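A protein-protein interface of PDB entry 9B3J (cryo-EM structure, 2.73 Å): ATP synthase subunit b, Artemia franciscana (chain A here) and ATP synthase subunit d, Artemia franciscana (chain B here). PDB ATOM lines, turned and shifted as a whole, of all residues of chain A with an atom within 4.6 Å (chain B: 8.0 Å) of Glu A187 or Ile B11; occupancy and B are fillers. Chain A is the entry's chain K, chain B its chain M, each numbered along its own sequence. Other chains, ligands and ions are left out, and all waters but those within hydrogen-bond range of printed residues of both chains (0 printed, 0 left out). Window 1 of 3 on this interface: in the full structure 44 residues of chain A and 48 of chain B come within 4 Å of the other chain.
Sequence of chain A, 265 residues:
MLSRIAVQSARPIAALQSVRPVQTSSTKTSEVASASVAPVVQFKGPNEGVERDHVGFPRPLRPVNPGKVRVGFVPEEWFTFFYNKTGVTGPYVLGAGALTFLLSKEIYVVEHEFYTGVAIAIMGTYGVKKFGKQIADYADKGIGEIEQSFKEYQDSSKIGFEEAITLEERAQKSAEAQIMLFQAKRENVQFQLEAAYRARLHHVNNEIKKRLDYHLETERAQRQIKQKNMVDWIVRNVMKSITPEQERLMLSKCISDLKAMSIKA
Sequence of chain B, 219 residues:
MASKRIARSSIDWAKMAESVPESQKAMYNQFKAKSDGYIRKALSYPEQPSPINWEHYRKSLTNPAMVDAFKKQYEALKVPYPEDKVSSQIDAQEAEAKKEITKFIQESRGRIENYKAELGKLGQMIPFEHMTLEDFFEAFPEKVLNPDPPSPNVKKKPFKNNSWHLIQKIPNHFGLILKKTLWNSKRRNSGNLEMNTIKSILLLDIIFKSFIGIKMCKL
Of the 9 printed residues of chain A, 8 touch a printed residue of chain B. Hydrophobic or aromatic side chains of chain A that line the printed part of chain B: Ala A184, Val A189 and Phe A191. Along chain A the printed residues that touch a printed residue of chain B span positions 183 to 191. Among the printed residues, no Asp or Glu carboxylate lies within 4 Å of a Lys or Arg side-chain nitrogen of the other chain.
Of the printed residues of chain B, Gln A183 touches Ile B11 (3.9 Å). Of chain B, only Ile B11 comes within 4 Å of Glu A187. Gln A190 touches none of the printed residues of chain B. Of the printed residues of chain A, Ser B9 touches Phe A191. Of the printed residues of chain A, Ile B11 touches Gln A183, Ala A184 and Glu A187. Printed residues of chain A within 4 Å of Ile B90: Arg A186 (3.7 Å) and Val A189 (3.8 Å).
The backbone carbonyl oxygen (O) of Ile B11 lies within hydrogen-bond range of the indole nitrogen (NE1) of Trp B13, 3.1 Å away. OE2 of Glu A187 sits close to NE2 of Gln A183 (3.4 Å). The backbone carbonyl oxygen (O) of Phe B31 sits at hydrogen-bond distance from the side-chain hydroxyl (OG) of Ser B35, at 2.5 Å.
Among the printed residues, pairs that only touch across the chains: Phe A191 with Arg B5 (3.1 Å), Phe A191 with Ile B6 (3.2 Å), Phe A191 with Ser B9 (3.2 Å), Asn A188 with Tyr B38 (3.3 Å), Asn A188 with Ser B35 (3.4 Å), Lys A185 with Phe B31 (3.6 Å), Arg A186 with Ile B90 (3.7 Å), Glu A187 with Ile B11 (3.7 Å), Val A189 with Ile B90 (3.8 Å), Ala A184 with Ile B11 (3.8 Å), Ala A184 with Phe B31 (3.9 Å) and Gln A183 with Ile B11 (3.9 Å).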
ATOM      1  N   GLN A 183      23.596  36.422  -8.023  1.00  0.00           N
ATOM      2  CA  GLN A 183      22.568  35.482  -8.464  1.00  0.00           C
ATOM      3  C   GLN A 183      23.190  34.218  -9.055  1.00  0.00           C
ATOM      4  O   GLN A 183      22.708  33.103  -8.810  1.00  0.00           O
ATOM      5  CB  GLN A 183      21.647  36.158  -9.477  1.00  0.00           C
ATOM      6  CG  GLN A 183      20.275  35.522  -9.601  1.00  0.00           C
ATOM      7  CD  GLN A 183      20.254  34.334 -10.540  1.00  0.00           C
ATOM      8  OE1 GLN A 183      21.149  34.163 -11.366  1.00  0.00           O
ATOM      9  NE2 GLN A 183      19.226  33.505 -10.418  1.00  0.00           N
ATOM     10  N   ALA A 184      24.266  34.376  -9.835  1.00  0.00           N
ATOM     11  CA  ALA A 184      24.974  33.217 -10.369  1.00  0.00           C
ATOM     12  C   ALA A 184      25.653  32.417  -9.267  1.00  0.00           C
ATOM     13  O   ALA A 184      25.807  31.199  -9.393  1.00  0.00           O
ATOM     14  CB  ALA A 184      26.004  33.660 -11.405  1.00  0.00           C
ATOM     15  N   LYS A 185      26.056  33.082  -8.185  1.00  0.00           N
ATOM     16  CA  LYS A 185      26.652  32.382  -7.052  1.00  0.00           C
ATOM     17  C   LYS A 185      25.641  31.451  -6.395  1.00  0.00           C
ATOM     18  O   LYS A 185      25.928  30.267  -6.153  1.00  0.00           O
ATOM     19  CB  LYS A 185      27.188  33.391  -6.035  1.00  0.00           C
ATOM     20  CG  LYS A 185      28.546  33.972  -6.380  1.00  0.00           C
ATOM     21  CD  LYS A 185      28.991  34.976  -5.332  1.00  0.00           C
ATOM     22  CE  LYS A 185      30.400  35.476  -5.602  1.00  0.00           C
ATOM     23  NZ  LYS A 185      30.854  36.437  -4.560  1.00  0.00           N
ATOM     24  N   ARG A 186      24.442  31.968  -6.111  1.00  0.00           N
ATOM     25  CA  ARG A 186      23.441  31.121  -5.461  1.00  0.00           C
ATOM     26  C   ARG A 186      22.903  30.050  -6.407  1.00  0.00           C
ATOM     27  O   ARG A 186      22.545  28.944  -5.961  1.00  0.00           O
ATOM     28  CB  ARG A 186      22.308  31.970  -4.884  1.00  0.00           C
ATOM     29  CG  ARG A 186      21.327  32.552  -5.885  1.00  0.00           C
ATOM     30  CD  ARG A 186      20.287  33.402  -5.173  1.00  0.00           C
ATOM     31  NE  ARG A 186      19.172  33.754  -6.043  1.00  0.00           N
ATOM     32  CZ  ARG A 186      18.039  33.070  -6.118  1.00  0.00           C
ATOM     33  NH1 ARG A 186      17.835  31.991  -5.382  1.00  0.00           N
ATOM     34  NH2 ARG A 186      17.088  33.479  -6.952  1.00  0.00           N
ATOM     35  N   GLU A 187      22.880  30.334  -7.715  1.00  0.00           N
ATOM     36  CA  GLU A 187      22.536  29.296  -8.680  1.00  0.00           C
ATOM     37  C   GLU A 187      23.582  28.189  -8.698  1.00  0.00           C
ATOM     38  O   GLU A 187      23.237  27.006  -8.773  1.00  0.00           O
ATOM     39  CB  GLU A 187      22.376  29.901 -10.073  1.00  0.00           C
ATOM     40  CG  GLU A 187      21.059  30.624 -10.295  1.00  0.00           C
ATOM     41  CD  GLU A 187      19.918  29.679 -10.624  1.00  0.00           C
ATOM     42  OE1 GLU A 187      20.189  28.491 -10.897  1.00  0.00           O
ATOM     43  OE2 GLU A 187      18.752  30.126 -10.612  1.00  0.00           O
ATOM     44  N   ASN A 188      24.865  28.556  -8.619  1.00  0.00           N
ATOM     45  CA  ASN A 188      25.929  27.559  -8.640  1.00  0.00           C
ATOM     46  C   ASN A 188      25.902  26.689  -7.391  1.00  0.00           C
ATOM     47  O   ASN A 188      26.205  25.489  -7.457  1.00  0.00           O
ATOM     48  CB  ASN A 188      27.283  28.252  -8.785  1.00  0.00           C
ATOM     49  CG  ASN A 188      28.410  27.278  -9.053  1.00  0.00           C
ATOM     50  OD1 ASN A 188      28.184  26.169  -9.537  1.00  0.00           O
ATOM     51  ND2 ASN A 188      29.635  27.687  -8.738  1.00  0.00           N
ATOM     52  N   VAL A 189      25.544  27.276  -6.246  1.00  0.00           N
ATOM     53  CA  VAL A 189      25.430  26.494  -5.015  1.00  0.00           C
ATOM     54  C   VAL A 189      24.302  25.473  -5.127  1.00  0.00           C
ATOM     55  O   VAL A 189      24.459  24.304  -4.735  1.00  0.00           O
ATOM     56  CB  VAL A 189      25.235  27.431  -3.810  1.00  0.00           C
ATOM     57  CG1 VAL A 189      24.903  26.639  -2.551  1.00  0.00           C
ATOM     58  CG2 VAL A 189      26.484  28.264  -3.596  1.00  0.00           C
ATOM     59  N   GLN A 190      23.151  25.895  -5.670  1.00  0.00           N
ATOM     60  CA  GLN A 190      22.051  24.953  -5.875  1.00  0.00           C
ATOM     61  C   GLN A 190      22.422  23.861  -6.878  1.00  0.00           C
ATOM     62  O   GLN A 190      22.014  22.702  -6.724  1.00  0.00           O
ATOM     63  CB  GLN A 190      20.802  25.698  -6.336  1.00  0.00           C
ATOM     64  CG  GLN A 190      20.239  26.659  -5.306  1.00  0.00           C
ATOM     65  CD  GLN A 190      19.064  27.456  -5.839  1.00  0.00           C
ATOM     66  OE1 GLN A 190      18.513  27.139  -6.895  1.00  0.00           O
ATOM     67  NE2 GLN A 190      18.677  28.497  -5.112  1.00  0.00           N
ATOM     68  N   PHE A 191      23.190  24.218  -7.912  1.00  0.00           N
ATOM     69  CA  PHE A 191      23.653  23.228  -8.881  1.00  0.00           C
ATOM     70  C   PHE A 191      24.568  22.199  -8.232  1.00  0.00           C
ATOM     71  O   PHE A 191      24.466  21.000  -8.515  1.00  0.00           O
ATOM     72  CB  PHE A 191      24.378  23.918 -10.035  1.00  0.00           C
ATOM     73  CG  PHE A 191      23.503  24.211 -11.220  1.00  0.00           C
ATOM     74  CD1 PHE A 191      22.475  25.136 -11.132  1.00  0.00           C
ATOM     75  CD2 PHE A 191      23.719  23.575 -12.430  1.00  0.00           C
ATOM     76  CE1 PHE A 191      21.677  25.417 -12.226  1.00  0.00           C
ATOM     77  CE2 PHE A 191      22.924  23.852 -13.527  1.00  0.00           C
ATOM     78  CZ  PHE A 191      21.900  24.771 -13.421  1.00  0.00           C
ATOM     79  N   ARG B   5      17.519  21.597 -13.255  1.00  0.00           N
ATOM     80  CA  ARG B   5      18.413  22.601 -12.697  1.00  0.00           C
ATOM     81  C   ARG B   5      19.823  22.069 -12.472  1.00  0.00           C
ATOM     82  O   ARG B   5      20.535  22.581 -11.603  1.00  0.00           O
ATOM     83  CB  ARG B   5      17.847  23.148 -11.383  1.00  0.00           C
ATOM     84  CG  ARG B   5      16.364  23.474 -11.412  1.00  0.00           C
ATOM     85  CD  ARG B   5      15.583  22.518 -10.522  1.00  0.00           C
ATOM     86  NE  ARG B   5      16.091  22.509  -9.155  1.00  0.00           N
ATOM     87  CZ  ARG B   5      15.699  21.664  -8.211  1.00  0.00           C
ATOM     88  NH1 ARG B   5      14.784  20.739  -8.449  1.00  0.00           N
ATOM     89  NH2 ARG B   5      16.242  21.746  -7.000  1.00  0.00           N
ATOM     90  N   ILE B   6      20.225  21.032 -13.204  1.00  0.00           N
ATOM     91  CA  ILE B   6      21.592  20.524 -13.141  1.00  0.00           C
ATOM     92  C   ILE B   6      22.165  20.448 -14.552  1.00  0.00           C
ATOM     93  O   ILE B   6      23.252  20.971 -14.821  1.00  0.00           O
ATOM     94  CB  ILE B   6      21.660  19.163 -12.413  1.00  0.00           C
ATOM     95  CG1 ILE B   6      22.893  18.364 -12.841  1.00  0.00           C
ATOM     96  CG2 ILE B   6      20.400  18.354 -12.630  1.00  0.00           C
ATOM     97  CD1 ILE B   6      23.247  17.223 -11.920  1.00  0.00           C
ATOM     98  N   SER B   9      20.459  23.997 -17.505  1.00  0.00           N
ATOM     99  CA  SER B   9      20.294  25.369 -17.051  1.00  0.00           C
ATOM    100  C   SER B   9      21.661  25.963 -16.751  1.00  0.00           C
ATOM    101  O   SER B   9      22.625  25.242 -16.479  1.00  0.00           O
ATOM    102  CB  SER B   9      19.387  25.453 -15.817  1.00  0.00           C
ATOM    103  OG  SER B   9      19.287  26.786 -15.348  1.00  0.00           O
ATOM    104  N   SER B  10      21.730  27.291 -16.801  1.00  0.00           N
ATOM    105  CA  SER B  10      22.960  28.034 -16.547  1.00  0.00           C
ATOM    106  C   SER B  10      22.596  29.491 -16.276  1.00  0.00           C
ATOM    107  O   SER B  10      21.417  29.848 -16.180  1.00  0.00           O
ATOM    108  CB  SER B  10      23.935  27.909 -17.722  1.00  0.00           C
ATOM    109  OG  SER B  10      25.111  28.662 -17.484  1.00  0.00           O
ATOM    110  N   ILE B  11      23.619  30.335 -16.152  1.00  0.00           N
ATOM    111  CA  ILE B  11      23.465  31.774 -15.976  1.00  0.00           C
ATOM    112  C   ILE B  11      24.155  32.460 -17.145  1.00  0.00           C
ATOM    113  O   ILE B  11      25.231  32.030 -17.575  1.00  0.00           O
ATOM    114  CB  ILE B  11      24.050  32.263 -14.633  1.00  0.00           C
ATOM    115  CG1 ILE B  11      23.601  31.362 -13.482  1.00  0.00           C
ATOM    116  CG2 ILE B  11      23.633  33.696 -14.351  1.00  0.00           C
ATOM    117  CD1 ILE B  11      24.682  30.429 -12.975  1.00  0.00           C
ATOM    118  N   ASP B  12      23.529  33.512 -17.666  1.00  0.00           N
ATOM    119  CA  ASP B  12      24.046  34.218 -18.836  1.00  0.00           C
ATOM    120  C   ASP B  12      25.353  34.918 -18.490  1.00  0.00           C
ATOM    121  O   ASP B  12      25.363  35.907 -17.751  1.00  0.00           O
ATOM    122  CB  ASP B  12      23.015  35.221 -19.342  1.00  0.00           C
ATOM    123  CG  ASP B  12      23.546  36.079 -20.468  1.00  0.00           C
ATOM    124  OD1 ASP B  12      23.723  35.552 -21.586  1.00  0.00           O
ATOM    125  OD2 ASP B  12      23.793  37.281 -20.236  1.00  0.00           O
ATOM    126  N   TRP B  13      26.460  34.406 -19.027  1.00  0.00           N
ATOM    127  CA  TRP B  13      27.765  35.015 -18.819  1.00  0.00           C
ATOM    128  C   TRP B  13      28.049  36.148 -19.792  1.00  0.00           C
ATOM    129  O   TRP B  13      29.059  36.840 -19.626  1.00  0.00           O
ATOM    130  CB  TRP B  13      28.869  33.965 -18.948  1.00  0.00           C
ATOM    131  CG  TRP B  13      28.569  32.677 -18.259  1.00  0.00           C
ATOM    132  CD1 TRP B  13      28.018  31.562 -18.815  1.00  0.00           C
ATOM    133  CD2 TRP B  13      28.812  32.363 -16.884  1.00  0.00           C
ATOM    134  NE1 TRP B  13      27.897  30.574 -17.870  1.00  0.00           N
ATOM    135  CE2 TRP B  13      28.380  31.041 -16.676  1.00  0.00           C
ATOM    136  CE3 TRP B  13      29.353  33.072 -15.810  1.00  0.00           C
ATOM    137  CZ2 TRP B  13      28.470  30.413 -15.438  1.00  0.00           C
ATOM    138  CZ3 TRP B  13      29.441  32.448 -14.582  1.00  0.00           C
ATOM    139  CH2 TRP B  13      29.004  31.133 -14.405  1.00  0.00           C
ATOM    140  N   ALA B  14      27.198  36.336 -20.804  1.00  0.00           N
ATOM    141  CA  ALA B  14      27.451  37.353 -21.821  1.00  0.00           C
ATOM    142  C   ALA B  14      27.402  38.756 -21.234  1.00  0.00           C
ATOM    143  O   ALA B  14      28.261  39.592 -21.535  1.00  0.00           O
ATOM    144  CB  ALA B  14      26.444  37.212 -22.961  1.00  0.00           C
ATOM    145  N   LYS B  15      26.412  39.031 -20.385  1.00  0.00           N
ATOM    146  CA  LYS B  15      26.345  40.320 -19.713  1.00  0.00           C
ATOM    147  C   LYS B  15      27.344  40.431 -18.573  1.00  0.00           C
ATOM    148  O   LYS B  15      27.601  41.542 -18.096  1.00  0.00           O
ATOM    149  CB  LYS B  15      24.930  40.565 -19.189  1.00  0.00           C
ATOM    150  CG  LYS B  15      23.880  40.620 -20.282  1.00  0.00           C
ATOM    151  CD  LYS B  15      22.511  40.968 -19.725  1.00  0.00           C
ATOM    152  CE  LYS B  15      21.490  41.118 -20.842  1.00  0.00           C
ATOM    153  NZ  LYS B  15      20.146  41.489 -20.323  1.00  0.00           N
ATOM    154  N   MET B  16      27.911  39.308 -18.128  1.00  0.00           N
ATOM    155  CA  MET B  16      28.896  39.346 -17.056  1.00  0.00           C
ATOM    156  C   MET B  16      30.238  39.867 -17.553  1.00  0.00           C
ATOM    157  O   MET B  16      30.926  40.611 -16.844  1.00  0.00           O
ATOM    158  CB  MET B  16      29.054  37.956 -16.448  1.00  0.00           C
ATOM    159  CG  MET B  16      29.904  37.937 -15.203  1.00  0.00           C
ATOM    160  SD  MET B  16      29.963  36.317 -14.435  1.00  0.00           S
ATOM    161  CE  MET B  16      30.750  36.740 -12.887  1.00  0.00           C
ATOM    162  N   PHE B  31      35.734  32.180 -11.715  1.00  0.00           N
ATOM    163  CA  PHE B  31      34.311  31.957 -11.479  1.00  0.00           C
ATOM    164  C   PHE B  31      33.642  31.319 -12.687  1.00  0.00           C
ATOM    165  O   PHE B  31      32.751  30.475 -12.536  1.00  0.00           O
ATOM    166  CB  PHE B  31      33.619  33.271 -11.122  1.00  0.00           C
ATOM    167  CG  PHE B  31      32.193  33.103 -10.686  1.00  0.00           C
ATOM    168  CD1 PHE B  31      31.898  32.730  -9.387  1.00  0.00           C
ATOM    169  CD2 PHE B  31      31.149  33.318 -11.570  1.00  0.00           C
ATOM    170  CE1 PHE B  31      30.588  32.572  -8.980  1.00  0.00           C
ATOM    171  CE2 PHE B  31      29.836  33.163 -11.167  1.00  0.00           C
ATOM    172  CZ  PHE B  31      29.556  32.791  -9.871  1.00  0.00           C
ATOM    173  N   LYS B  32      34.053  31.709 -13.891  1.00  0.00           N
ATOM    174  CA  LYS B  32      33.551  31.043 -15.082  1.00  0.00           C
ATOM    175  C   LYS B  32      34.109  29.633 -15.217  1.00  0.00           C
ATOM    176  O   LYS B  32      33.491  28.799 -15.885  1.00  0.00           O
ATOM    177  CB  LYS B  32      33.884  31.872 -16.324  1.00  0.00           C
ATOM    178  CG  LYS B  32      32.837  31.805 -17.428  1.00  0.00           C
ATOM    179  CD  LYS B  32      33.182  30.760 -18.473  1.00  0.00           C
ATOM    180  CE  LYS B  32      32.120  30.695 -19.557  1.00  0.00           C
ATOM    181  NZ  LYS B  32      32.442  29.672 -20.588  1.00  0.00           N
ATOM    182  N   SER B  35      32.813  27.204 -11.594  1.00  0.00           N
ATOM    183  CA  SER B  35      31.419  26.832 -11.801  1.00  0.00           C
ATOM    184  C   SER B  35      31.270  25.889 -12.983  1.00  0.00           C
ATOM    185  O   SER B  35      30.383  25.026 -12.974  1.00  0.00           O
ATOM    186  CB  SER B  35      30.565  28.081 -12.006  1.00  0.00           C
ATOM    187  OG  SER B  35      31.004  28.805 -13.140  1.00  0.00           O
ATOM    188  N   TYR B  38      31.452  22.571 -11.738  1.00  0.00           N
ATOM    189  CA  TYR B  38      30.130  22.154 -11.295  1.00  0.00           C
ATOM    190  C   TYR B  38      29.165  21.966 -12.456  1.00  0.00           C
ATOM    191  O   TYR B  38      28.067  21.438 -12.247  1.00  0.00           O
ATOM    192  CB  TYR B  38      29.569  23.167 -10.301  1.00  0.00           C
ATOM    193  CG  TYR B  38      30.468  23.391  -9.111  1.00  0.00           C
ATOM    194  CD1 TYR B  38      30.735  22.363  -8.220  1.00  0.00           C
ATOM    195  CD2 TYR B  38      31.048  24.630  -8.878  1.00  0.00           C
ATOM    196  CE1 TYR B  38      31.556  22.561  -7.129  1.00  0.00           C
ATOM    197  CE2 TYR B  38      31.872  24.839  -7.789  1.00  0.00           C
ATOM    198  CZ  TYR B  38      32.121  23.801  -6.917  1.00  0.00           C
ATOM    199  OH  TYR B  38      32.941  24.001  -5.831  1.00  0.00           O
ATOM    200  N   ILE B  39      29.536  22.401 -13.659  1.00  0.00           N
ATOM    201  CA  ILE B  39      28.821  21.993 -14.859  1.00  0.00           C
ATOM    202  C   ILE B  39      29.385  20.677 -15.395  1.00  0.00           C
ATOM    203  O   ILE B  39      28.633  19.848 -15.922  1.00  0.00           O
ATOM    204  CB  ILE B  39      28.879  23.116 -15.914  1.00  0.00           C
ATOM    205  CG1 ILE B  39      28.275  24.406 -15.355  1.00  0.00           C
ATOM    206  CG2 ILE B  39      28.135  22.736 -17.188  1.00  0.00           C
ATOM    207  CD1 ILE B  39      28.393  25.589 -16.295  1.00  0.00           C
ATOM    208  N   ILE B  90      24.399  33.589   1.748  1.00  0.00           N
ATOM    209  CA  ILE B  90      24.311  34.241   0.445  1.00  0.00           C
ATOM    210  C   ILE B  90      23.347  35.420   0.501  1.00  0.00           C
ATOM    211  O   ILE B  90      23.597  36.467  -0.104  1.00  0.00           O
ATOM    212  CB  ILE B  90      23.916  33.207  -0.626  1.00  0.00           C
ATOM    213  CG1 ILE B  90      25.077  32.237  -0.858  1.00  0.00           C
ATOM    214  CG2 ILE B  90      23.518  33.873  -1.933  1.00  0.00           C
ATOM    215  CD1 ILE B  90      24.776  31.149  -1.857  1.00  0.00           C
